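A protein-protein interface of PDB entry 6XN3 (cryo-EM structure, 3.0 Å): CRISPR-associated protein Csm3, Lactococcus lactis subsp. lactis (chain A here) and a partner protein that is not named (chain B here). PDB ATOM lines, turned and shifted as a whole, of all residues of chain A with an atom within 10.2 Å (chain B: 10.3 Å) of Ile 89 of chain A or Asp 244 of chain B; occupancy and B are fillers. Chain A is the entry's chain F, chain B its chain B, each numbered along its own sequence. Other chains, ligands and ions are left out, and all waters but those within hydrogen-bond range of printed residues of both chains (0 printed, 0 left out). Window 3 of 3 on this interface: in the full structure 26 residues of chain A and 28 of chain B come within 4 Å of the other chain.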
ATOM      1  N   ASP A  75     -11.050  28.140 -23.884  1.00  0.00           N
ATOM      2  CA  ASP A  75      -9.759  28.782 -23.655  1.00  0.00           C
ATOM      3  C   ASP A  75      -9.918  30.030 -22.791  1.00  0.00           C
ATOM      4  O   ASP A  75      -9.029  30.357 -21.999  1.00  0.00           O
ATOM      5  CB  ASP A  75      -9.127  29.094 -25.025  1.00  0.00           C
ATOM      6  CG  ASP A  75      -7.662  29.582 -24.961  1.00  0.00           C
ATOM      7  OD1 ASP A  75      -7.269  30.450 -24.161  1.00  0.00           O
ATOM      8  OD2 ASP A  75      -6.881  29.111 -25.812  1.00  0.00           O
ATOM      9  N   LEU A  78     -10.247  28.900 -18.966  1.00  0.00           N
ATOM     10  CA  LEU A  78      -8.975  28.398 -18.460  1.00  0.00           C
ATOM     11  C   LEU A  78      -7.950  29.514 -18.361  1.00  0.00           C
ATOM     12  O   LEU A  78      -7.149  29.546 -17.421  1.00  0.00           O
ATOM     13  CB  LEU A  78      -8.455  27.278 -19.352  1.00  0.00           C
ATOM     14  CG  LEU A  78      -9.295  26.008 -19.393  1.00  0.00           C
ATOM     15  CD1 LEU A  78      -8.693  25.018 -20.363  1.00  0.00           C
ATOM     16  CD2 LEU A  78      -9.425  25.402 -18.018  1.00  0.00           C
ATOM     17  N   ARG A  79      -7.970  30.452 -19.303  1.00  0.00           N
ATOM     18  CA  ARG A  79      -7.029  31.555 -19.240  1.00  0.00           C
ATOM     19  C   ARG A  79      -7.414  32.586 -18.194  1.00  0.00           C
ATOM     20  O   ARG A  79      -6.561  33.379 -17.792  1.00  0.00           O
ATOM     21  CB  ARG A  79      -6.883  32.206 -20.617  1.00  0.00           C
ATOM     22  CG  ARG A  79      -7.700  33.450 -20.858  1.00  0.00           C
ATOM     23  CD  ARG A  79      -7.728  33.767 -22.337  1.00  0.00           C
ATOM     24  NE  ARG A  79      -8.676  34.821 -22.675  1.00  0.00           N
ATOM     25  CZ  ARG A  79      -9.084  35.087 -23.909  1.00  0.00           C
ATOM     26  NH1 ARG A  79      -8.631  34.375 -24.928  1.00  0.00           N
ATOM     27  NH2 ARG A  79      -9.949  36.063 -24.125  1.00  0.00           N
ATOM     28  N   PHE A  81      -9.069  31.549 -15.079  1.00  0.00           N
ATOM     29  CA  PHE A  81      -9.015  30.925 -13.759  1.00  0.00           C
ATOM     30  C   PHE A  81      -8.087  29.718 -13.688  1.00  0.00           C
ATOM     31  O   PHE A  81      -8.217  28.880 -12.798  1.00  0.00           O
ATOM     32  CB  PHE A  81     -10.410  30.526 -13.298  1.00  0.00           C
ATOM     33  CG  PHE A  81     -11.406  31.633 -13.369  1.00  0.00           C
ATOM     34  CD1 PHE A  81     -11.452  32.597 -12.384  1.00  0.00           C
ATOM     35  CD2 PHE A  81     -12.309  31.701 -14.406  1.00  0.00           C
ATOM     36  CE1 PHE A  81     -12.365  33.615 -12.441  1.00  0.00           C
ATOM     37  CE2 PHE A  81     -13.228  32.717 -14.464  1.00  0.00           C
ATOM     38  CZ  PHE A  81     -13.257  33.673 -13.479  1.00  0.00           C
ATOM     39  N   GLY A  82      -7.140  29.607 -14.602  1.00  0.00           N
ATOM     40  CA  GLY A  82      -6.145  28.561 -14.471  1.00  0.00           C
ATOM     41  C   GLY A  82      -6.601  27.213 -15.001  1.00  0.00           C
ATOM     42  O   GLY A  82      -7.754  27.004 -15.366  1.00  0.00           O
ATOM     43  N   SER A  83      -5.653  26.281 -15.013  1.00  0.00           N
ATOM     44  CA  SER A  83      -5.857  24.964 -15.597  1.00  0.00           C
ATOM     45  C   SER A  83      -4.757  24.034 -15.121  1.00  0.00           C
ATOM     46  O   SER A  83      -3.585  24.410 -15.071  1.00  0.00           O
ATOM     47  CB  SER A  83      -5.847  25.028 -17.120  1.00  0.00           C
ATOM     48  OG  SER A  83      -4.623  25.577 -17.568  1.00  0.00           O
ATOM     49  N   SER A  84      -5.145  22.808 -14.785  1.00  0.00           N
ATOM     50  CA  SER A  84      -4.167  21.763 -14.521  1.00  0.00           C
ATOM     51  C   SER A  84      -4.476  20.502 -15.313  1.00  0.00           C
ATOM     52  O   SER A  84      -4.229  19.400 -14.807  1.00  0.00           O
ATOM     53  CB  SER A  84      -4.098  21.421 -13.040  1.00  0.00           C
ATOM     54  OG  SER A  84      -5.067  20.441 -12.719  1.00  0.00           O
ATOM     55  N   GLU A  85      -5.036  20.635 -16.513  1.00  0.00           N
ATOM     56  CA  GLU A  85      -5.306  19.498 -17.380  1.00  0.00           C
ATOM     57  C   GLU A  85      -3.993  18.850 -17.805  1.00  0.00           C
ATOM     58  O   GLU A  85      -2.955  19.508 -17.876  1.00  0.00           O
ATOM     59  CB  GLU A  85      -6.106  19.976 -18.595  1.00  0.00           C
ATOM     60  CG  GLU A  85      -6.674  18.906 -19.508  1.00  0.00           C
ATOM     61  CD  GLU A  85      -7.383  19.495 -20.708  1.00  0.00           C
ATOM     62  OE1 GLU A  85      -7.816  18.723 -21.585  1.00  0.00           O
ATOM     63  OE2 GLU A  85      -7.526  20.732 -20.767  1.00  0.00           O
ATOM     64  N   LYS A  86      -4.050  17.540 -18.059  1.00  0.00           N
ATOM     65  CA  LYS A  86      -2.848  16.758 -18.339  1.00  0.00           C
ATOM     66  C   LYS A  86      -2.162  17.201 -19.624  1.00  0.00           C
ATOM     67  O   LYS A  86      -0.939  17.093 -19.751  1.00  0.00           O
ATOM     68  CB  LYS A  86      -3.191  15.274 -18.417  1.00  0.00           C
ATOM     69  CG  LYS A  86      -3.580  14.628 -17.107  1.00  0.00           C
ATOM     70  CD  LYS A  86      -4.027  13.204 -17.377  1.00  0.00           C
ATOM     71  CE  LYS A  86      -2.851  12.326 -17.780  1.00  0.00           C
ATOM     72  NZ  LYS A  86      -3.240  10.898 -17.944  1.00  0.00           N
ATOM     73  N   ASP A  87      -2.928  17.681 -20.600  1.00  0.00           N
ATOM     74  CA  ASP A  87      -2.272  18.126 -21.820  1.00  0.00           C
ATOM     75  C   ASP A  87      -1.891  19.597 -21.772  1.00  0.00           C
ATOM     76  O   ASP A  87      -0.726  19.939 -21.991  1.00  0.00           O
ATOM     77  CB  ASP A  87      -3.157  17.858 -23.036  1.00  0.00           C
ATOM     78  CG  ASP A  87      -2.346  17.529 -24.283  1.00  0.00           C
ATOM     79  OD1 ASP A  87      -1.325  18.206 -24.533  1.00  0.00           O
ATOM     80  OD2 ASP A  87      -2.724  16.585 -25.009  1.00  0.00           O
ATOM     81  N   LYS A  88      -2.840  20.478 -21.476  1.00  0.00           N
ATOM     82  CA  LYS A  88      -2.602  21.914 -21.510  1.00  0.00           C
ATOM     83  C   LYS A  88      -2.658  22.466 -20.092  1.00  0.00           C
ATOM     84  O   LYS A  88      -3.555  22.121 -19.316  1.00  0.00           O
ATOM     85  CB  LYS A  88      -3.600  22.610 -22.446  1.00  0.00           C
ATOM     86  CG  LYS A  88      -5.068  22.437 -22.100  1.00  0.00           C
ATOM     87  CD  LYS A  88      -5.981  22.938 -23.201  1.00  0.00           C
ATOM     88  CE  LYS A  88      -6.031  21.943 -24.349  1.00  0.00           C
ATOM     89  NZ  LYS A  88      -7.087  22.269 -25.343  1.00  0.00           N
ATOM     90  N   ILE A  89      -1.655  23.259 -19.737  1.00  0.00           N
ATOM     91  CA  ILE A  89      -1.580  23.931 -18.449  1.00  0.00           C
ATOM     92  C   ILE A  89      -1.381  25.408 -18.723  1.00  0.00           C
ATOM     93  O   ILE A  89      -0.492  25.787 -19.493  1.00  0.00           O
ATOM     94  CB  ILE A  89      -0.427  23.399 -17.575  1.00  0.00           C
ATOM     95  CG1 ILE A  89      -0.472  21.883 -17.452  1.00  0.00           C
ATOM     96  CG2 ILE A  89      -0.476  24.021 -16.202  1.00  0.00           C
ATOM     97  CD1 ILE A  89       0.733  21.310 -16.770  1.00  0.00           C
ATOM     98  N   ARG A  90      -2.206  26.246 -18.108  1.00  0.00           N
ATOM     99  CA  ARG A  90      -2.049  27.679 -18.263  1.00  0.00           C
ATOM    100  C   ARG A  90      -2.061  28.333 -16.893  1.00  0.00           C
ATOM    101  O   ARG A  90      -2.810  27.930 -16.002  1.00  0.00           O
ATOM    102  CB  ARG A  90      -3.137  28.275 -19.148  1.00  0.00           C
ATOM    103  CG  ARG A  90      -2.774  29.628 -19.727  1.00  0.00           C
ATOM    104  CD  ARG A  90      -3.792  30.096 -20.748  1.00  0.00           C
ATOM    105  NE  ARG A  90      -3.845  29.220 -21.912  1.00  0.00           N
ATOM    106  CZ  ARG A  90      -4.845  28.385 -22.168  1.00  0.00           C
ATOM    107  NH1 ARG A  90      -5.864  28.306 -21.329  1.00  0.00           N
ATOM    108  NH2 ARG A  90      -4.820  27.620 -23.247  1.00  0.00           N
ATOM    109  N   ARG A  91      -1.197  29.326 -16.733  1.00  0.00           N
ATOM    110  CA  ARG A  91      -1.130  30.096 -15.505  1.00  0.00           C
ATOM    111  C   ARG A  91      -2.393  30.926 -15.362  1.00  0.00           C
ATOM    112  O   ARG A  91      -2.876  31.501 -16.339  1.00  0.00           O
ATOM    113  CB  ARG A  91       0.099  30.995 -15.525  1.00  0.00           C
ATOM    114  CG  ARG A  91       0.508  31.560 -14.187  1.00  0.00           C
ATOM    115  CD  ARG A  91       1.620  32.600 -14.332  1.00  0.00           C
ATOM    116  NE  ARG A  91       2.805  32.085 -15.020  1.00  0.00           N
ATOM    117  CZ  ARG A  91       3.154  32.404 -16.265  1.00  0.00           C
ATOM    118  NH1 ARG A  91       2.406  33.239 -16.968  1.00  0.00           N
ATOM    119  NH2 ARG A  91       4.245  31.882 -16.805  1.00  0.00           N
ATOM    120  N   ALA A  92      -2.937  30.969 -14.152  1.00  0.00           N
ATOM    121  CA  ALA A  92      -4.153  31.726 -13.903  1.00  0.00           C
ATOM    122  C   ALA A  92      -3.874  33.214 -13.990  1.00  0.00           C
ATOM    123  O   ALA A  92      -3.004  33.725 -13.281  1.00  0.00           O
ATOM    124  CB  ALA A  92      -4.730  31.385 -12.533  1.00  0.00           C
ATOM    125  N   ARG A  93      -4.586  33.912 -14.867  1.00  0.00           N
ATOM    126  CA  ARG A  93      -4.429  35.356 -14.936  1.00  0.00           C
ATOM    127  C   ARG A  93      -5.002  36.054 -13.716  1.00  0.00           C
ATOM    128  O   ARG A  93      -4.390  37.004 -13.220  1.00  0.00           O
ATOM    129  CB  ARG A  93      -5.081  35.894 -16.205  1.00  0.00           C
ATOM    130  CG  ARG A  93      -4.237  35.669 -17.436  1.00  0.00           C
ATOM    131  CD  ARG A  93      -4.931  36.132 -18.692  1.00  0.00           C
ATOM    132  NE  ARG A  93      -4.084  35.928 -19.859  1.00  0.00           N
ATOM    133  CZ  ARG A  93      -4.500  36.053 -21.111  1.00  0.00           C
ATOM    134  NH1 ARG A  93      -5.757  36.378 -21.364  1.00  0.00           N
ATOM    135  NH2 ARG A  93      -3.659  35.844 -22.112  1.00  0.00           N
ATOM    136  N   ASN A 151      -3.377  39.634 -14.160  1.00  0.00           N
ATOM    137  CA  ASN A 151      -2.035  39.543 -14.723  1.00  0.00           C
ATOM    138  C   ASN A 151      -2.088  39.957 -16.186  1.00  0.00           C
ATOM    139  O   ASN A 151      -2.391  39.139 -17.057  1.00  0.00           O
ATOM    140  CB  ASN A 151      -1.494  38.127 -14.578  1.00  0.00           C
ATOM    141  CG  ASN A 151       0.009  38.064 -14.667  1.00  0.00           C
ATOM    142  OD1 ASN A 151       0.647  38.937 -15.245  1.00  0.00           O
ATOM    143  ND2 ASN A 151       0.589  37.031 -14.077  1.00  0.00           N
ATOM    144  N   ASP A 153      -0.685  39.937 -18.975  1.00  0.00           N
ATOM    145  CA  ASP A 153       0.380  39.291 -19.722  1.00  0.00           C
ATOM    146  C   ASP A 153       0.211  39.421 -21.227  1.00  0.00           C
ATOM    147  O   ASP A 153       1.200  39.332 -21.962  1.00  0.00           O
ATOM    148  CB  ASP A 153       0.503  37.819 -19.294  1.00  0.00           C
ATOM    149  CG  ASP A 153      -0.751  36.988 -19.574  1.00  0.00           C
ATOM    150  OD1 ASP A 153      -1.776  37.508 -20.064  1.00  0.00           O
ATOM    151  OD2 ASP A 153      -0.709  35.775 -19.286  1.00  0.00           O
ATOM    152  N   ILE B  37       9.966  33.164 -10.978  1.00  0.00           N
ATOM    153  CA  ILE B  37       8.737  33.032 -11.754  1.00  0.00           C
ATOM    154  C   ILE B  37       8.185  34.411 -12.093  1.00  0.00           C
ATOM    155  O   ILE B  37       7.662  34.639 -13.192  1.00  0.00           O
ATOM    156  CB  ILE B  37       7.713  32.128 -11.034  1.00  0.00           C
ATOM    157  CG1 ILE B  37       6.571  31.740 -11.971  1.00  0.00           C
ATOM    158  CG2 ILE B  37       7.119  32.752  -9.815  1.00  0.00           C
ATOM    159  CD1 ILE B  37       6.985  30.870 -13.119  1.00  0.00           C
ATOM    160  N   VAL B  40      10.559  35.859 -14.981  1.00  0.00           N
ATOM    161  CA  VAL B  40      10.231  35.374 -16.318  1.00  0.00           C
ATOM    162  C   VAL B  40       8.845  35.878 -16.701  1.00  0.00           C
ATOM    163  O   VAL B  40       8.499  35.945 -17.887  1.00  0.00           O
ATOM    164  CB  VAL B  40      10.358  33.833 -16.401  1.00  0.00           C
ATOM    165  CG1 VAL B  40       9.421  33.134 -15.454  1.00  0.00           C
ATOM    166  CG2 VAL B  40      10.244  33.294 -17.837  1.00  0.00           C
ATOM    167  N   GLY B  41       8.042  36.281 -15.709  1.00  0.00           N
ATOM    168  CA  GLY B  41       6.912  37.149 -16.004  1.00  0.00           C
ATOM    169  C   GLY B  41       7.326  38.460 -16.652  1.00  0.00           C
ATOM    170  O   GLY B  41       6.665  38.943 -17.573  1.00  0.00           O
ATOM    171  N   PHE B 240       6.678  20.115  -6.886  1.00  0.00           N
ATOM    172  CA  PHE B 240       6.355  20.073  -8.299  1.00  0.00           C
ATOM    173  C   PHE B 240       6.835  21.344  -8.973  1.00  0.00           C
ATOM    174  O   PHE B 240       6.899  22.406  -8.353  1.00  0.00           O
ATOM    175  CB  PHE B 240       4.860  19.933  -8.524  1.00  0.00           C
ATOM    176  CG  PHE B 240       4.359  18.539  -8.403  1.00  0.00           C
ATOM    177  CD1 PHE B 240       4.340  17.907  -7.183  1.00  0.00           C
ATOM    178  CD2 PHE B 240       3.898  17.860  -9.513  1.00  0.00           C
ATOM    179  CE1 PHE B 240       3.882  16.634  -7.077  1.00  0.00           C
ATOM    180  CE2 PHE B 240       3.431  16.573  -9.406  1.00  0.00           C
ATOM    181  CZ  PHE B 240       3.425  15.958  -8.187  1.00  0.00           C
ATOM    182  N   VAL B 241       7.169  21.231 -10.246  1.00  0.00           N
ATOM    183  CA  VAL B 241       7.587  22.396 -11.008  1.00  0.00           C
ATOM    184  C   VAL B 241       6.359  23.230 -11.336  1.00  0.00           C
ATOM    185  O   VAL B 241       5.421  22.746 -11.978  1.00  0.00           O
ATOM    186  CB  VAL B 241       8.324  21.976 -12.283  1.00  0.00           C
ATOM    187  CG1 VAL B 241       8.755  23.197 -13.037  1.00  0.00           C
ATOM    188  CG2 VAL B 241       9.509  21.119 -11.936  1.00  0.00           C
ATOM    189  N   GLN B 242       6.361  24.484 -10.901  1.00  0.00           N
ATOM    190  CA  GLN B 242       5.253  25.399 -11.148  1.00  0.00           C
ATOM    191  C   GLN B 242       5.610  26.257 -12.349  1.00  0.00           C
ATOM    192  O   GLN B 242       6.213  27.322 -12.206  1.00  0.00           O
ATOM    193  CB  GLN B 242       4.963  26.264  -9.931  1.00  0.00           C
ATOM    194  CG  GLN B 242       3.760  27.160 -10.107  1.00  0.00           C
ATOM    195  CD  GLN B 242       3.652  28.187  -9.018  1.00  0.00           C
ATOM    196  OE1 GLN B 242       3.953  27.908  -7.867  1.00  0.00           O
ATOM    197  NE2 GLN B 242       3.241  29.390  -9.378  1.00  0.00           N
ATOM    198  N   SER B 243       5.243  25.783 -13.533  1.00  0.00           N
ATOM    199  CA  SER B 243       5.350  26.575 -14.746  1.00  0.00           C
ATOM    200  C   SER B 243       4.410  25.989 -15.778  1.00  0.00           C
ATOM    201  O   SER B 243       3.908  24.874 -15.628  1.00  0.00           O
ATOM    202  CB  SER B 243       6.771  26.599 -15.298  1.00  0.00           C
ATOM    203  OG  SER B 243       7.139  25.310 -15.726  1.00  0.00           O
ATOM    204  N   ASP B 244       4.183  26.762 -16.831  1.00  0.00           N
ATOM    205  CA  ASP B 244       3.430  26.320 -17.989  1.00  0.00           C
ATOM    206  C   ASP B 244       4.325  25.959 -19.165  1.00  0.00           C
ATOM    207  O   ASP B 244       3.843  25.842 -20.295  1.00  0.00           O
ATOM    208  CB  ASP B 244       2.397  27.386 -18.366  1.00  0.00           C
ATOM    209  CG  ASP B 244       3.023  28.729 -18.772  1.00  0.00           C
ATOM    210  OD1 ASP B 244       4.259  28.908 -18.739  1.00  0.00           O
ATOM    211  OD2 ASP B 244       2.245  29.634 -19.134  1.00  0.00           O
ATOM    212  N   THR B 245       5.622  25.790 -18.922  1.00  0.00           N
ATOM    213  CA  THR B 245       6.586  25.586 -19.990  1.00  0.00           C
ATOM    214  C   THR B 245       7.429  24.336 -19.756  1.00  0.00           C
ATOM    215  O   THR B 245       7.944  23.756 -20.719  1.00  0.00           O
ATOM    216  CB  THR B 245       7.473  26.832 -20.121  1.00  0.00           C
ATOM    217  OG1 THR B 245       6.650  27.997 -20.020  1.00  0.00           O
ATOM    218  CG2 THR B 245       8.161  26.886 -21.472  1.00  0.00           C
ATOM    219  N   TYR B 246       7.543  23.872 -18.520  1.00  0.00           N
ATOM    220  CA  TYR B 246       8.342  22.693 -18.201  1.00  0.00           C
ATOM    221  C   TYR B 246       7.532  21.451 -18.539  1.00  0.00           C
ATOM    222  O   TYR B 246       6.800  20.933 -17.696  1.00  0.00           O
ATOM    223  CB  TYR B 246       8.747  22.692 -16.732  1.00  0.00           C
ATOM    224  CG  TYR B 246       9.841  21.720 -16.351  1.00  0.00           C
ATOM    225  CD1 TYR B 246       9.562  20.387 -16.089  1.00  0.00           C
ATOM    226  CD2 TYR B 246      11.151  22.148 -16.219  1.00  0.00           C
ATOM    227  CE1 TYR B 246      10.556  19.511 -15.734  1.00  0.00           C
ATOM    228  CE2 TYR B 246      12.151  21.279 -15.857  1.00  0.00           C
ATOM    229  CZ  TYR B 246      11.847  19.963 -15.619  1.00  0.00           C
ATOM    230  OH  TYR B 246      12.846  19.090 -15.261  1.00  0.00           O
ATOM    231  N   ALA B 247       7.652  21.001 -19.786  1.00  0.00           N
ATOM    232  CA  ALA B 247       7.407  19.621 -20.204  1.00  0.00           C
ATOM    233  C   ALA B 247       5.975  19.138 -19.987  1.00  0.00           C
ATOM    234  O   ALA B 247       5.775  18.083 -19.383  1.00  0.00           O
ATOM    235  CB  ALA B 247       8.379  18.664 -19.508  1.00  0.00           C
ATOM    236  N   THR B 248       4.977  19.904 -20.448  1.00  0.00           N
ATOM    237  CA  THR B 248       3.573  19.541 -20.710  1.00  0.00           C
ATOM    238  C   THR B 248       2.847  18.714 -19.647  1.00  0.00           C
ATOM    239  O   THR B 248       1.818  18.102 -19.943  1.00  0.00           O
ATOM    240  CB  THR B 248       3.402  18.828 -22.075  1.00  0.00           C
ATOM    241  OG1 THR B 248       2.005  18.644 -22.326  1.00  0.00           O
ATOM    242  CG2 THR B 248       4.062  17.439 -22.171  1.00  0.00           C
ATOM    243  N   ASN B 249       3.312  18.760 -18.401  1.00  0.00           N
ATOM    244  CA  ASN B 249       2.734  17.975 -17.319  1.00  0.00           C
ATOM    245  C   ASN B 249       3.128  18.603 -15.996  1.00  0.00           C
ATOM    246  O   ASN B 249       3.660  19.712 -15.941  1.00  0.00           O
ATOM    247  CB  ASN B 249       3.198  16.521 -17.350  1.00  0.00           C
ATOM    248  CG  ASN B 249       2.325  15.658 -18.198  1.00  0.00           C
ATOM    249  OD1 ASN B 249       1.105  15.774 -18.157  1.00  0.00           O
ATOM    250  ND2 ASN B 249       2.938  14.791 -18.988  1.00  0.00           N
ATOM    251  N   LEU B 250       2.860  17.866 -14.922  1.00  0.00           N
ATOM    252  CA  LEU B 250       3.300  18.258 -13.589  1.00  0.00           C
ATOM    253  C   LEU B 250       4.395  17.291 -13.162  1.00  0.00           C
ATOM    254  O   LEU B 250       4.155  16.236 -12.573  1.00  0.00           O
ATOM    255  CB  LEU B 250       2.134  18.269 -12.617  1.00  0.00           C
ATOM    256  CG  LEU B 250       0.956  19.121 -13.063  1.00  0.00           C
ATOM    257  CD1 LEU B 250      -0.272  18.698 -12.316  1.00  0.00           C
ATOM    258  CD2 LEU B 250       1.247  20.578 -12.820  1.00  0.00           C
ATOM    259  N   VAL B 251       5.617  17.659 -13.484  1.00  0.00           N
ATOM    260  CA  VAL B 251       6.775  16.835 -13.185  1.00  0.00           C
ATOM    261  C   VAL B 251       7.337  17.252 -11.837  1.00  0.00           C
ATOM    262  O   VAL B 251       7.447  18.445 -11.541  1.00  0.00           O
ATOM    263  CB  VAL B 251       7.816  16.980 -14.304  1.00  0.00           C
ATOM    264  CG1 VAL B 251       9.025  16.115 -14.040  1.00  0.00           C
ATOM    265  CG2 VAL B 251       7.188  16.641 -15.634  1.00  0.00           C
ATOM    266  N   GLY B 280      12.931  19.445 -18.590  1.00  0.00           N
ATOM    267  CA  GLY B 280      11.918  20.236 -19.248  1.00  0.00           C
ATOM    268  C   GLY B 280      12.498  21.118 -20.333  1.00  0.00           C
ATOM    269  O   GLY B 280      13.583  20.884 -20.866  1.00  0.00           O
ATOM    270  N   ASN B 281      11.740  22.159 -20.667  1.00  0.00           N
ATOM    271  CA  ASN B 281      12.157  23.089 -21.703  1.00  0.00           C
ATOM    272  C   ASN B 281      12.929  24.283 -21.160  1.00  0.00           C
ATOM    273  O   ASN B 281      13.371  25.125 -21.947  1.00  0.00           O
ATOM    274  CB  ASN B 281      10.939  23.567 -22.483  1.00  0.00           C
ATOM    275  CG  ASN B 281      10.463  22.543 -23.484  1.00  0.00           C
ATOM    276  OD1 ASN B 281      10.966  21.422 -23.523  1.00  0.00           O
ATOM    277  ND2 ASN B 281       9.496  22.922 -24.307  1.00  0.00           N
ATOM    278  N   HIS B 282      13.096  24.379 -19.848  1.00  0.00           N
ATOM    279  CA  HIS B 282      13.836  25.445 -19.201  1.00  0.00           C
ATOM    280  C   HIS B 282      14.394  24.891 -17.902  1.00  0.00           C
ATOM    281  O   HIS B 282      13.805  23.968 -17.330  1.00  0.00           O
ATOM    282  CB  HIS B 282      12.928  26.655 -18.930  1.00  0.00           C
ATOM    283  CG  HIS B 282      11.843  26.384 -17.939  1.00  0.00           C
ATOM    284  ND1 HIS B 282      12.022  26.522 -16.581  1.00  0.00           N
ATOM    285  CD2 HIS B 282      10.561  25.985 -18.112  1.00  0.00           C
ATOM    286  CE1 HIS B 282      10.897  26.218 -15.959  1.00  0.00           C
ATOM    287  NE2 HIS B 282       9.995  25.888 -16.865  1.00  0.00           N
ATOM    288  N   VAL B 284      15.283  24.511 -13.925  1.00  0.00           N
ATOM    289  CA  VAL B 284      14.619  24.813 -12.664  1.00  0.00           C
ATOM    290  C   VAL B 284      15.687  24.877 -11.592  1.00  0.00           C
ATOM    291  O   VAL B 284      16.351  23.873 -11.311  1.00  0.00           O
ATOM    292  CB  VAL B 284      13.557  23.766 -12.308  1.00  0.00           C
ATOM    293  CG1 VAL B 284      13.046  23.998 -10.908  1.00  0.00           C
ATOM    294  CG2 VAL B 284      12.427  23.839 -13.289  1.00  0.00           C
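Asp 244 of chain B touches Ile 89 of chain A. Asn 249 of chain B touches Ile 89 of chain A (O to CD1, 3.4 Å).
Of chain A, only Ile 89 (3.5 Å) and Arg 91 (3.5 Å) come within 4 Å of Asp 244 of chain B. No residue of chain B comes within 4 Å of Arg 90 of chain A. Of chain B, only Asp 244 (3.5 Å) comes within 4 Å of Arg 91 of chain A. No residue of chain A comes within 4 Å of Ser 243 of chain B. Thr 245 of chain B touches none of the printed residues of chain A. Printed residues of chain B within 4 Å of Asp 87 of chain A: Thr 248. Printed residues of chain A within 4 Å of Asn 249 of chain B: Lys 86 (2.9 Å) and Ile 89 (3.4 Å). Printed residues of chain A within 4 Å of Thr 248 of chain B: Lys 86 (2.9 Å) and Asp 87 (3.0 Å). The nearest residue of chain A that does not touch Asp 244 of chain B is Arg 90 of chain A (4.5 Å).
OD1 of Asp 244 of chain B is in salt-bridge range of NH2 of Arg 91 of chain A (3.5 Å). O of Thr 248 of chain B lies close to O of Lys 86 of chain A. OG1 of Thr 248 of chain B lies within hydrogen-bond range of O of Asp 87 of chain A (3.0 Å). The side-chain amide oxygen of Asn 249 of chain B lies close to the backbone carbonyl oxygen of Lys 86 of chain A, at 2.9 Å.
Of the 19 printed residues of chain B, 3 touch a printed residue of chain A. Printed residues of chain A that touch a printed residue of chain B: Lys 86, Asp 87, Ile 89 and Arg 91. Hydrophobic or aromatic side chains of chain A within 4 Å of the printed part of chain B: Ile 89. Among the printed residues, 6 pairs touch across the chains.
OG1 of Thr 245 of chain B is in hydrogen-bond range of OD1 of Asp 244 of chain B, 2.9 Å away.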
